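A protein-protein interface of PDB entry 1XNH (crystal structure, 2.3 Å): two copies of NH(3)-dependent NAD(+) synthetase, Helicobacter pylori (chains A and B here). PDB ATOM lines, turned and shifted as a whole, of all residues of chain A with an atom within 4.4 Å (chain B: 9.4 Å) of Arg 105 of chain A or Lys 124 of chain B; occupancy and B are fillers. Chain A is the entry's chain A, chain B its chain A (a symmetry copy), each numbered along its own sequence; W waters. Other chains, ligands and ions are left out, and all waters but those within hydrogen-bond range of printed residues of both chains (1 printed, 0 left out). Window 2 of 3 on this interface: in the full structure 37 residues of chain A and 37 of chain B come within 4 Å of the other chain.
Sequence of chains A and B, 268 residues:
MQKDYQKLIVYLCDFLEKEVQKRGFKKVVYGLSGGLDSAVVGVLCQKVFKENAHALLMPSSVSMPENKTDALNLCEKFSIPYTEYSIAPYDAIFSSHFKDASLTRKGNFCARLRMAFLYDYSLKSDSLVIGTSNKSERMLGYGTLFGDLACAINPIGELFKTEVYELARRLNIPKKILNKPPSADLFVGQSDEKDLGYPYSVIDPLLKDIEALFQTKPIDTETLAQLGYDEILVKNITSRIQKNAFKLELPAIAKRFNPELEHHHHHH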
ATOM      1  N   PHE A  94       7.432  -1.837  -6.467  1.00  0.00           N
ATOM      2  CA  PHE A  94       6.059  -2.053  -6.039  1.00  0.00           C
ATOM      3  C   PHE A  94       5.135  -1.859  -7.233  1.00  0.00           C
ATOM      4  O   PHE A  94       4.221  -2.660  -7.473  1.00  0.00           O
ATOM      5  CB  PHE A  94       5.713  -1.076  -4.903  1.00  0.00           C
ATOM      6  CG  PHE A  94       4.282  -1.130  -4.458  1.00  0.00           C
ATOM      7  CD1 PHE A  94       3.378  -0.155  -4.864  1.00  0.00           C
ATOM      8  CD2 PHE A  94       3.827  -2.169  -3.654  1.00  0.00           C
ATOM      9  CE1 PHE A  94       2.032  -0.223  -4.478  1.00  0.00           C
ATOM     10  CE2 PHE A  94       2.483  -2.244  -3.267  1.00  0.00           C
ATOM     11  CZ  PHE A  94       1.590  -1.267  -3.682  1.00  0.00           C
ATOM     12  N   PHE A  98       2.704  -4.205  -9.118  1.00  0.00           N
ATOM     13  CA  PHE A  98       1.326  -3.778  -8.900  1.00  0.00           C
ATOM     14  C   PHE A  98       0.969  -2.551  -9.744  1.00  0.00           C
ATOM     15  O   PHE A  98       1.125  -1.415  -9.301  1.00  0.00           O
ATOM     16  CB  PHE A  98       1.106  -3.471  -7.409  1.00  0.00           C
ATOM     17  CG  PHE A  98       1.055  -4.697  -6.535  1.00  0.00           C
ATOM     18  CD1 PHE A  98       1.653  -4.699  -5.282  1.00  0.00           C
ATOM     19  CD2 PHE A  98       0.407  -5.853  -6.966  1.00  0.00           C
ATOM     20  CE1 PHE A  98       1.613  -5.839  -4.467  1.00  0.00           C
ATOM     21  CE2 PHE A  98       0.360  -6.997  -6.160  1.00  0.00           C
ATOM     22  CZ  PHE A  98       0.965  -6.987  -4.906  1.00  0.00           C
ATOM     23  N   ALA A 101      -2.494  -0.981  -8.610  1.00  0.00           N
ATOM     24  CA  ALA A 101      -2.464  -0.505  -7.245  1.00  0.00           C
ATOM     25  C   ALA A 101      -3.089   0.879  -7.110  1.00  0.00           C
ATOM     26  O   ALA A 101      -2.692   1.814  -7.805  1.00  0.00           O
ATOM     27  CB  ALA A 101      -1.033  -0.485  -6.749  1.00  0.00           C
ATOM     28  N   SER A 102      -4.065   1.011  -6.213  1.00  0.00           N
ATOM     29  CA  SER A 102      -4.757   2.284  -5.994  1.00  0.00           C
ATOM     30  C   SER A 102      -3.839   3.321  -5.368  1.00  0.00           C
ATOM     31  O   SER A 102      -2.737   3.005  -4.924  1.00  0.00           O
ATOM     32  CB  SER A 102      -5.959   2.079  -5.082  1.00  0.00           C
ATOM     33  OG  SER A 102      -5.548   1.650  -3.798  1.00  0.00           O
ATOM     34  N   LEU A 103      -4.309   4.561  -5.317  1.00  0.00           N
ATOM     35  CA  LEU A 103      -3.515   5.644  -4.756  1.00  0.00           C
ATOM     36  C   LEU A 103      -3.138   5.301  -3.313  1.00  0.00           C
ATOM     37  O   LEU A 103      -1.950   5.195  -2.979  1.00  0.00           O
ATOM     38  CB  LEU A 103      -4.307   6.957  -4.782  1.00  0.00           C
ATOM     39  CG  LEU A 103      -4.842   7.512  -6.120  1.00  0.00           C
ATOM     40  CD1 LEU A 103      -5.807   8.668  -5.844  1.00  0.00           C
ATOM     41  CD2 LEU A 103      -3.685   7.983  -6.997  1.00  0.00           C
ATOM     42  N   THR A 104      -4.155   5.104  -2.475  1.00  0.00           N
ATOM     43  CA  THR A 104      -3.958   4.782  -1.072  1.00  0.00           C
ATOM     44  C   THR A 104      -3.004   3.610  -0.865  1.00  0.00           C
ATOM     45  O   THR A 104      -2.180   3.627   0.062  1.00  0.00           O
ATOM     46  CB  THR A 104      -5.312   4.465  -0.395  1.00  0.00           C
ATOM     47  OG1 THR A 104      -6.192   5.595  -0.526  1.00  0.00           O
ATOM     48  CG2 THR A 104      -5.111   4.144   1.090  1.00  0.00           C
ATOM     49  N   ARG A 105      -3.095   2.591  -1.716  1.00  0.00           N
ATOM     50  CA  ARG A 105      -2.208   1.440  -1.571  1.00  0.00           C
ATOM     51  C   ARG A 105      -0.751   1.852  -1.692  1.00  0.00           C
ATOM     52  O   ARG A 105       0.067   1.452  -0.870  1.00  0.00           O
ATOM     53  CB  ARG A 105      -2.554   0.350  -2.600  1.00  0.00           C
ATOM     54  CG  ARG A 105      -3.856  -0.369  -2.250  1.00  0.00           C
ATOM     55  CD  ARG A 105      -4.141  -1.500  -3.177  1.00  0.00           C
ATOM     56  NE  ARG A 105      -3.027  -2.417  -3.220  1.00  0.00           N
ATOM     57  CZ  ARG A 105      -2.878  -3.358  -4.137  1.00  0.00           C
ATOM     58  NH1 ARG A 105      -3.783  -3.495  -5.082  1.00  0.00           N
ATOM     59  NH2 ARG A 105      -1.821  -4.162  -4.096  1.00  0.00           N
ATOM     60  N   LYS A 106      -0.446   2.659  -2.708  1.00  0.00           N
ATOM     61  CA  LYS A 106       0.903   3.154  -2.952  1.00  0.00           C
ATOM     62  C   LYS A 106       1.339   4.106  -1.819  1.00  0.00           C
ATOM     63  O   LYS A 106       2.525   4.162  -1.430  1.00  0.00           O
ATOM     64  CB  LYS A 106       0.954   3.905  -4.282  1.00  0.00           C
ATOM     65  CG  LYS A 106       0.381   3.122  -5.476  1.00  0.00           C
ATOM     66  CD  LYS A 106       0.598   3.904  -6.773  1.00  0.00           C
ATOM     67  CE  LYS A 106       1.690   3.273  -7.615  1.00  0.00           C
ATOM     68  NZ  LYS A 106       1.261   1.977  -8.208  1.00  0.00           N
ATOM     69  N   GLY A 107       0.375   4.861  -1.301  1.00  0.00           N
ATOM     70  CA  GLY A 107       0.645   5.781  -0.219  1.00  0.00           C
ATOM     71  C   GLY A 107       0.990   5.026   1.068  1.00  0.00           C
ATOM     72  O   GLY A 107       1.909   5.400   1.764  1.00  0.00           O
ATOM     73  N   ASN A 108       0.243   3.975   1.398  1.00  0.00           N
ATOM     74  CA  ASN A 108       0.497   3.218   2.609  1.00  0.00           C
ATOM     75  C   ASN A 108       1.886   2.560   2.553  1.00  0.00           C
ATOM     76  O   ASN A 108       2.683   2.632   3.520  1.00  0.00           O
ATOM     77  CB  ASN A 108      -0.605   2.188   2.807  1.00  0.00           C
ATOM     78  CG  ASN A 108      -1.939   2.856   3.109  1.00  0.00           C
ATOM     79  OD1 ASN A 108      -1.969   4.062   3.350  1.00  0.00           O
ATOM     80  ND2 ASN A 108      -3.029   2.093   3.121  1.00  0.00           N
ATOM     81  N   PHE A 109       2.185   1.935   1.415  1.00  0.00           N
ATOM     82  CA  PHE A 109       3.470   1.285   1.205  1.00  0.00           C
ATOM     83  C   PHE A 109       4.645   2.237   1.400  1.00  0.00           C
ATOM     84  O   PHE A 109       5.582   1.919   2.121  1.00  0.00           O
ATOM     85  CB  PHE A 109       3.547   0.730  -0.197  1.00  0.00           C
ATOM     86  CG  PHE A 109       4.757  -0.102  -0.430  1.00  0.00           C
ATOM     87  CD1 PHE A 109       4.942  -1.272   0.289  1.00  0.00           C
ATOM     88  CD2 PHE A 109       5.720   0.273  -1.360  1.00  0.00           C
ATOM     89  CE1 PHE A 109       6.059  -2.063   0.094  1.00  0.00           C
ATOM     90  CE2 PHE A 109       6.844  -0.512  -1.564  1.00  0.00           C
ATOM     91  CZ  PHE A 109       7.011  -1.682  -0.836  1.00  0.00           C
ATOM     92  N   PHE B  25     -14.964  -7.649   9.577  1.00  0.00           N
ATOM     93  CA  PHE B  25     -14.267  -8.446   8.588  1.00  0.00           C
ATOM     94  C   PHE B  25     -14.734  -9.890   8.608  1.00  0.00           C
ATOM     95  O   PHE B  25     -15.391 -10.323   9.559  1.00  0.00           O
ATOM     96  CB  PHE B  25     -12.759  -8.400   8.855  1.00  0.00           C
ATOM     97  CG  PHE B  25     -12.174  -7.013   8.811  1.00  0.00           C
ATOM     98  CD1 PHE B  25     -12.317  -6.149   9.892  1.00  0.00           C
ATOM     99  CD2 PHE B  25     -11.494  -6.565   7.679  1.00  0.00           C
ATOM    100  CE1 PHE B  25     -11.788  -4.855   9.851  1.00  0.00           C
ATOM    101  CE2 PHE B  25     -10.963  -5.278   7.624  1.00  0.00           C
ATOM    102  CZ  PHE B  25     -11.114  -4.419   8.718  1.00  0.00           C
ATOM    103  N   LYS B  27     -12.490 -12.051   6.504  1.00  0.00           N
ATOM    104  CA  LYS B  27     -11.288 -12.636   5.913  1.00  0.00           C
ATOM    105  C   LYS B  27     -10.058 -12.203   6.726  1.00  0.00           C
ATOM    106  O   LYS B  27     -10.052 -11.135   7.331  1.00  0.00           O
ATOM    107  CB  LYS B  27     -11.164 -12.170   4.451  1.00  0.00           C
ATOM    108  CG  LYS B  27     -12.061 -12.936   3.464  1.00  0.00           C
ATOM    109  CD  LYS B  27     -11.976 -12.413   2.028  1.00  0.00           C
ATOM    110  CE  LYS B  27     -12.852 -11.177   1.836  1.00  0.00           C
ATOM    111  NZ  LYS B  27     -12.887 -10.676   0.428  1.00  0.00           N
ATOM    112  N   VAL B  29      -5.451 -12.551   6.892  1.00  0.00           N
ATOM    113  CA  VAL B  29      -4.236 -12.906   6.175  1.00  0.00           C
ATOM    114  C   VAL B  29      -3.107 -12.910   7.195  1.00  0.00           C
ATOM    115  O   VAL B  29      -3.198 -12.221   8.205  1.00  0.00           O
ATOM    116  CB  VAL B  29      -3.947 -11.854   5.089  1.00  0.00           C
ATOM    117  CG1 VAL B  29      -3.786 -10.511   5.750  1.00  0.00           C
ATOM    118  CG2 VAL B  29      -2.717 -12.245   4.279  1.00  0.00           C
ATOM    119  N   HIS B  54      -6.234 -16.404   4.479  1.00  0.00           N
ATOM    120  CA  HIS B  54      -5.188 -16.444   3.459  1.00  0.00           C
ATOM    121  C   HIS B  54      -3.775 -16.335   4.042  1.00  0.00           C
ATOM    122  O   HIS B  54      -3.537 -15.565   4.961  1.00  0.00           O
ATOM    123  CB  HIS B  54      -5.430 -15.305   2.452  1.00  0.00           C
ATOM    124  CG  HIS B  54      -4.854 -15.559   1.088  1.00  0.00           C
ATOM    125  ND1 HIS B  54      -3.646 -15.027   0.674  1.00  0.00           N
ATOM    126  CD2 HIS B  54      -5.314 -16.302   0.060  1.00  0.00           C
ATOM    127  CE1 HIS B  54      -3.398 -15.434  -0.549  1.00  0.00           C
ATOM    128  NE2 HIS B  54      -4.378 -16.207  -0.960  1.00  0.00           N
ATOM    129  N   LEU B  56       0.397 -15.693   3.243  1.00  0.00           N
ATOM    130  CA  LEU B  56       1.327 -14.971   2.373  1.00  0.00           C
ATOM    131  C   LEU B  56       2.764 -15.413   2.649  1.00  0.00           C
ATOM    132  O   LEU B  56       3.305 -15.134   3.722  1.00  0.00           O
ATOM    133  CB  LEU B  56       1.273 -13.467   2.629  1.00  0.00           C
ATOM    134  CG  LEU B  56       0.013 -12.682   2.239  1.00  0.00           C
ATOM    135  CD1 LEU B  56       0.284 -11.214   2.498  1.00  0.00           C
ATOM    136  CD2 LEU B  56      -0.330 -12.925   0.770  1.00  0.00           C
ATOM    137  N   THR B  83      -0.592 -16.808  -1.404  1.00  0.00           N
ATOM    138  CA  THR B  83       0.032 -16.010  -2.456  1.00  0.00           C
ATOM    139  C   THR B  83       1.533 -15.973  -2.219  1.00  0.00           C
ATOM    140  O   THR B  83       1.980 -15.675  -1.116  1.00  0.00           O
ATOM    141  CB  THR B  83      -0.491 -14.561  -2.465  1.00  0.00           C
ATOM    142  OG1 THR B  83      -1.884 -14.568  -2.811  1.00  0.00           O
ATOM    143  CG2 THR B  83       0.303 -13.690  -3.462  1.00  0.00           C
ATOM    144  N   TYR B  85       5.014 -14.235  -2.880  1.00  0.00           N
ATOM    145  CA  TYR B  85       5.605 -12.967  -3.306  1.00  0.00           C
ATOM    146  C   TYR B  85       6.950 -12.776  -2.605  1.00  0.00           C
ATOM    147  O   TYR B  85       7.007 -12.577  -1.387  1.00  0.00           O
ATOM    148  CB  TYR B  85       4.661 -11.801  -2.975  1.00  0.00           C
ATOM    149  CG  TYR B  85       5.112 -10.465  -3.539  1.00  0.00           C
ATOM    150  CD1 TYR B  85       4.982 -10.176  -4.903  1.00  0.00           C
ATOM    151  CD2 TYR B  85       5.718  -9.496  -2.720  1.00  0.00           C
ATOM    152  CE1 TYR B  85       5.452  -8.956  -5.437  1.00  0.00           C
ATOM    153  CE2 TYR B  85       6.182  -8.281  -3.257  1.00  0.00           C
ATOM    154  CZ  TYR B  85       6.047  -8.024  -4.609  1.00  0.00           C
ATOM    155  OH  TYR B  85       6.532  -6.827  -5.152  1.00  0.00           O
ATOM    156  N   ALA B 116       4.505  -4.661   5.338  1.00  0.00           N
ATOM    157  CA  ALA B 116       3.927  -3.750   4.371  1.00  0.00           C
ATOM    158  C   ALA B 116       2.991  -4.484   3.415  1.00  0.00           C
ATOM    159  O   ALA B 116       1.918  -4.002   3.077  1.00  0.00           O
ATOM    160  CB  ALA B 116       5.031  -3.043   3.586  1.00  0.00           C
ATOM    161  N   PHE B 117       3.408  -5.666   2.990  1.00  0.00           N
ATOM    162  CA  PHE B 117       2.616  -6.481   2.074  1.00  0.00           C
ATOM    163  C   PHE B 117       1.458  -7.209   2.720  1.00  0.00           C
ATOM    164  O   PHE B 117       0.496  -7.570   2.037  1.00  0.00           O
ATOM    165  CB  PHE B 117       3.496  -7.486   1.305  1.00  0.00           C
ATOM    166  CG  PHE B 117       4.502  -6.824   0.423  1.00  0.00           C
ATOM    167  CD1 PHE B 117       5.863  -6.889   0.719  1.00  0.00           C
ATOM    168  CD2 PHE B 117       4.090  -6.084  -0.676  1.00  0.00           C
ATOM    169  CE1 PHE B 117       6.807  -6.202  -0.051  1.00  0.00           C
ATOM    170  CE2 PHE B 117       5.023  -5.391  -1.457  1.00  0.00           C
ATOM    171  CZ  PHE B 117       6.375  -5.456  -1.149  1.00  0.00           C
ATOM    172  N   LEU B 118       1.536  -7.464   4.017  1.00  0.00           N
ATOM    173  CA  LEU B 118       0.418  -8.113   4.696  1.00  0.00           C
ATOM    174  C   LEU B 118      -0.642  -7.046   4.828  1.00  0.00           C
ATOM    175  O   LEU B 118      -1.822  -7.302   4.628  1.00  0.00           O
ATOM    176  CB  LEU B 118       0.832  -8.618   6.087  1.00  0.00           C
ATOM    177  CG  LEU B 118       1.443 -10.027   6.148  1.00  0.00           C
ATOM    178  CD1 LEU B 118       2.133 -10.265   7.495  1.00  0.00           C
ATOM    179  CD2 LEU B 118       0.358 -11.040   5.894  1.00  0.00           C
ATOM    180  N   TYR B 119      -0.227  -5.828   5.142  1.00  0.00           N
ATOM    181  CA  TYR B 119      -1.223  -4.774   5.278  1.00  0.00           C
ATOM    182  C   TYR B 119      -1.738  -4.218   3.940  1.00  0.00           C
ATOM    183  O   TYR B 119      -2.871  -3.734   3.879  1.00  0.00           O
ATOM    184  CB  TYR B 119      -0.728  -3.624   6.159  1.00  0.00           C
ATOM    185  CG  TYR B 119      -1.090  -3.840   7.613  1.00  0.00           C
ATOM    186  CD1 TYR B 119      -0.267  -4.582   8.455  1.00  0.00           C
ATOM    187  CD2 TYR B 119      -2.290  -3.332   8.138  1.00  0.00           C
ATOM    188  CE1 TYR B 119      -0.622  -4.814   9.773  1.00  0.00           C
ATOM    189  CE2 TYR B 119      -2.648  -3.557   9.455  1.00  0.00           C
ATOM    190  CZ  TYR B 119      -1.800  -4.304  10.270  1.00  0.00           C
ATOM    191  OH  TYR B 119      -2.133  -4.521  11.594  1.00  0.00           O
ATOM    192  N   ASP B 120      -0.911  -4.283   2.894  1.00  0.00           N
ATOM    193  CA  ASP B 120      -1.291  -3.866   1.549  1.00  0.00           C
ATOM    194  C   ASP B 120      -2.261  -4.956   1.055  1.00  0.00           C
ATOM    195  O   ASP B 120      -3.230  -4.677   0.367  1.00  0.00           O
ATOM    196  CB  ASP B 120      -0.044  -3.827   0.635  1.00  0.00           C
ATOM    197  CG  ASP B 120      -0.395  -3.727  -0.854  1.00  0.00           C
ATOM    198  OD1 ASP B 120      -0.660  -2.602  -1.329  1.00  0.00           O
ATOM    199  OD2 ASP B 120      -0.384  -4.769  -1.541  1.00  0.00           O
ATOM    200  N   TYR B 121      -1.987  -6.204   1.431  1.00  0.00           N
ATOM    201  CA  TYR B 121      -2.834  -7.309   1.004  1.00  0.00           C
ATOM    202  C   TYR B 121      -4.215  -7.236   1.683  1.00  0.00           C
ATOM    203  O   TYR B 121      -5.255  -7.515   1.059  1.00  0.00           O
ATOM    204  CB  TYR B 121      -2.196  -8.671   1.307  1.00  0.00           C
ATOM    205  CG  TYR B 121      -3.024  -9.848   0.794  1.00  0.00           C
ATOM    206  CD1 TYR B 121      -2.806 -10.389  -0.472  1.00  0.00           C
ATOM    207  CD2 TYR B 121      -4.075 -10.363   1.549  1.00  0.00           C
ATOM    208  CE1 TYR B 121      -3.627 -11.435  -0.979  1.00  0.00           C
ATOM    209  CE2 TYR B 121      -4.904 -11.395   1.063  1.00  0.00           C
ATOM    210  CZ  TYR B 121      -4.669 -11.927  -0.203  1.00  0.00           C
ATOM    211  OH  TYR B 121      -5.434 -12.992  -0.661  1.00  0.00           O
ATOM    212  N   SER B 122      -4.227  -6.846   2.955  1.00  0.00           N
ATOM    213  CA  SER B 122      -5.458  -6.702   3.716  1.00  0.00           C
ATOM    214  C   SER B 122      -6.299  -5.534   3.207  1.00  0.00           C
ATOM    215  O   SER B 122      -7.518  -5.568   3.288  1.00  0.00           O
ATOM    216  CB  SER B 122      -5.116  -6.485   5.185  1.00  0.00           C
ATOM    217  OG  SER B 122      -4.195  -5.426   5.290  1.00  0.00           O
ATOM    218  N   LEU B 123      -5.643  -4.489   2.713  1.00  0.00           N
ATOM    219  CA  LEU B 123      -6.357  -3.325   2.188  1.00  0.00           C
ATOM    220  C   LEU B 123      -7.202  -3.640   0.932  1.00  0.00           C
ATOM    221  O   LEU B 123      -8.360  -3.249   0.847  1.00  0.00           O
ATOM    222  CB  LEU B 123      -5.366  -2.217   1.841  1.00  0.00           C
ATOM    223  CG  LEU B 123      -5.902  -1.051   1.005  1.00  0.00           C
ATOM    224  CD1 LEU B 123      -7.146  -0.440   1.641  1.00  0.00           C
ATOM    225  CD2 LEU B 123      -4.817  -0.016   0.902  1.00  0.00           C
ATOM    226  N   LYS B 124      -6.608  -4.346  -0.025  1.00  0.00           N
ATOM    227  CA  LYS B 124      -7.264  -4.693  -1.279  1.00  0.00           C
ATOM    228  C   LYS B 124      -8.165  -5.923  -1.290  1.00  0.00           C
ATOM    229  O   LYS B 124      -8.828  -6.213  -2.292  1.00  0.00           O
ATOM    230  CB  LYS B 124      -6.217  -4.878  -2.381  1.00  0.00           C
ATOM    231  CG  LYS B 124      -5.276  -6.062  -2.129  1.00  0.00           C
ATOM    232  CD  LYS B 124      -4.336  -6.258  -3.318  1.00  0.00           C
ATOM    233  CE  LYS B 124      -3.255  -7.323  -3.072  1.00  0.00           C
ATOM    234  NZ  LYS B 124      -3.722  -8.731  -3.217  1.00  0.00           N
ATOM    235  N   SER B 125      -8.165  -6.672  -0.199  1.00  0.00           N
ATOM    236  CA  SER B 125      -8.986  -7.877  -0.103  1.00  0.00           C
ATOM    237  C   SER B 125      -9.896  -7.810   1.099  1.00  0.00           C
ATOM    238  O   SER B 125     -10.650  -8.738   1.348  1.00  0.00           O
ATOM    239  CB  SER B 125      -8.112  -9.144  -0.012  1.00  0.00           C
ATOM    240  OG  SER B 125      -7.296  -9.159   1.142  1.00  0.00           O
ATOM    241  N   ASP B 126      -9.804  -6.713   1.844  1.00  0.00           N
ATOM    242  CA  ASP B 126     -10.646  -6.507   3.011  1.00  0.00           C
ATOM    243  C   ASP B 126     -10.414  -7.585   4.057  1.00  0.00           C
ATOM    244  O   ASP B 126     -11.331  -8.331   4.412  1.00  0.00           O
ATOM    245  CB  ASP B 126     -12.119  -6.539   2.589  1.00  0.00           C
ATOM    246  CG  ASP B 126     -12.453  -5.501   1.533  1.00  0.00           C
ATOM    247  OD1 ASP B 126     -12.696  -4.333   1.900  1.00  0.00           O
ATOM    248  OD2 ASP B 126     -12.459  -5.855   0.333  1.00  0.00           O
ATOM    249  N   SER B 127      -9.184  -7.654   4.546  1.00  0.00           N
ATOM    250  CA  SER B 127      -8.811  -8.642   5.539  1.00  0.00           C
ATOM    251  C   SER B 127      -8.115  -8.042   6.763  1.00  0.00           C
ATOM    252  O   SER B 127      -7.684  -6.888   6.755  1.00  0.00           O
ATOM    253  CB  SER B 127      -7.875  -9.684   4.915  1.00  0.00           C
ATOM    254  OG  SER B 127      -8.559 -10.554   4.041  1.00  0.00           O
ATOM    255  N   LEU B 128      -8.026  -8.830   7.826  1.00  0.00           N
ATOM    256  CA  LEU B 128      -7.309  -8.357   8.994  1.00  0.00           C
ATOM    257  C   LEU B 128      -6.012  -9.163   9.134  1.00  0.00           C
ATOM    258  O   LEU B 128      -5.985 -10.365   8.862  1.00  0.00           O
ATOM    259  CB  LEU B 128      -8.137  -8.502  10.275  1.00  0.00           C
ATOM    260  CG  LEU B 128      -9.197  -7.433  10.557  1.00  0.00           C
ATOM    261  CD1 LEU B 128      -9.988  -7.845  11.798  1.00  0.00           C
ATOM    262  CD2 LEU B 128      -8.537  -6.063  10.743  1.00  0.00           C
HETATM  263  O   HOH W   1      -0.360  -0.755   0.623  1.00  0.00           O
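Hydrophobic or aromatic side chains of chain A within 4 Å of the printed part of chain B: Phe 94, Phe 98 and Phe 109.
Printed residues of chain B that touch a printed residue of chain A: Ala 116, Phe 117, Asp 120, Leu 123 and Lys 124.
Among the printed residues, 8 pairs touch across the chains.
N of Arg 105 of chain A lies close to OG of Ser 102 of chain A (3.4 Å).
OD1 of Asn 108 of chain A sits close to O of Thr 104 of chain A, at 3.3 Å.
No position is printed for both chains.
Printed residues of chain B within 4 Å of Phe 94 of chain A: Asp 120.
No residue of chain B comes within 4 Å of Thr 104 of chain A.
Of the printed residues of chain B, Asn 108 of chain A touches Leu 123.
Leu 118 of chain B touches none of the printed residues of chain A.
Lys 124 of chain B touches one residue of chain A.
Asp 126 of chain B touches none of the printed residues of chain A.
The nearest residue of chain B that does not touch Arg 105 of chain A is Tyr 121 of chain B (5.9 Å).
The nearest printed residue of chain A that does not touch Lys 124 of chain B is Phe 98 of chain A (4.6 Å).
Water W1 bridges the backbone carbonyl oxygen of Arg 105 of chain A (2.7 Å) and the side-chain carboxylate of Asp 120 of chain B (2.7 Å).
NH2 of Arg 105 of chain A is in salt-bridge range of OD2 of Asp 120 of chain B.
Among the printed residues, merely in contact across the chains: Phe 94 of chain A with Asp 120 of chain B (3.5 Å), Phe 98 of chain A with Asp 120 of chain B (3.7 Å), Arg 105 of chain A with Leu 123 of chain B (3.3 Å), Arg 105 of chain A with Lys 124 of chain B (3.3 Å), Asn 108 of chain A with Leu 123 of chain B (3.5 Å), Phe 109 of chain A with Ala 116 of chain B (3.7 Å) and Phe 109 of chain A with Phe 117 of chain B (3.6 Å).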
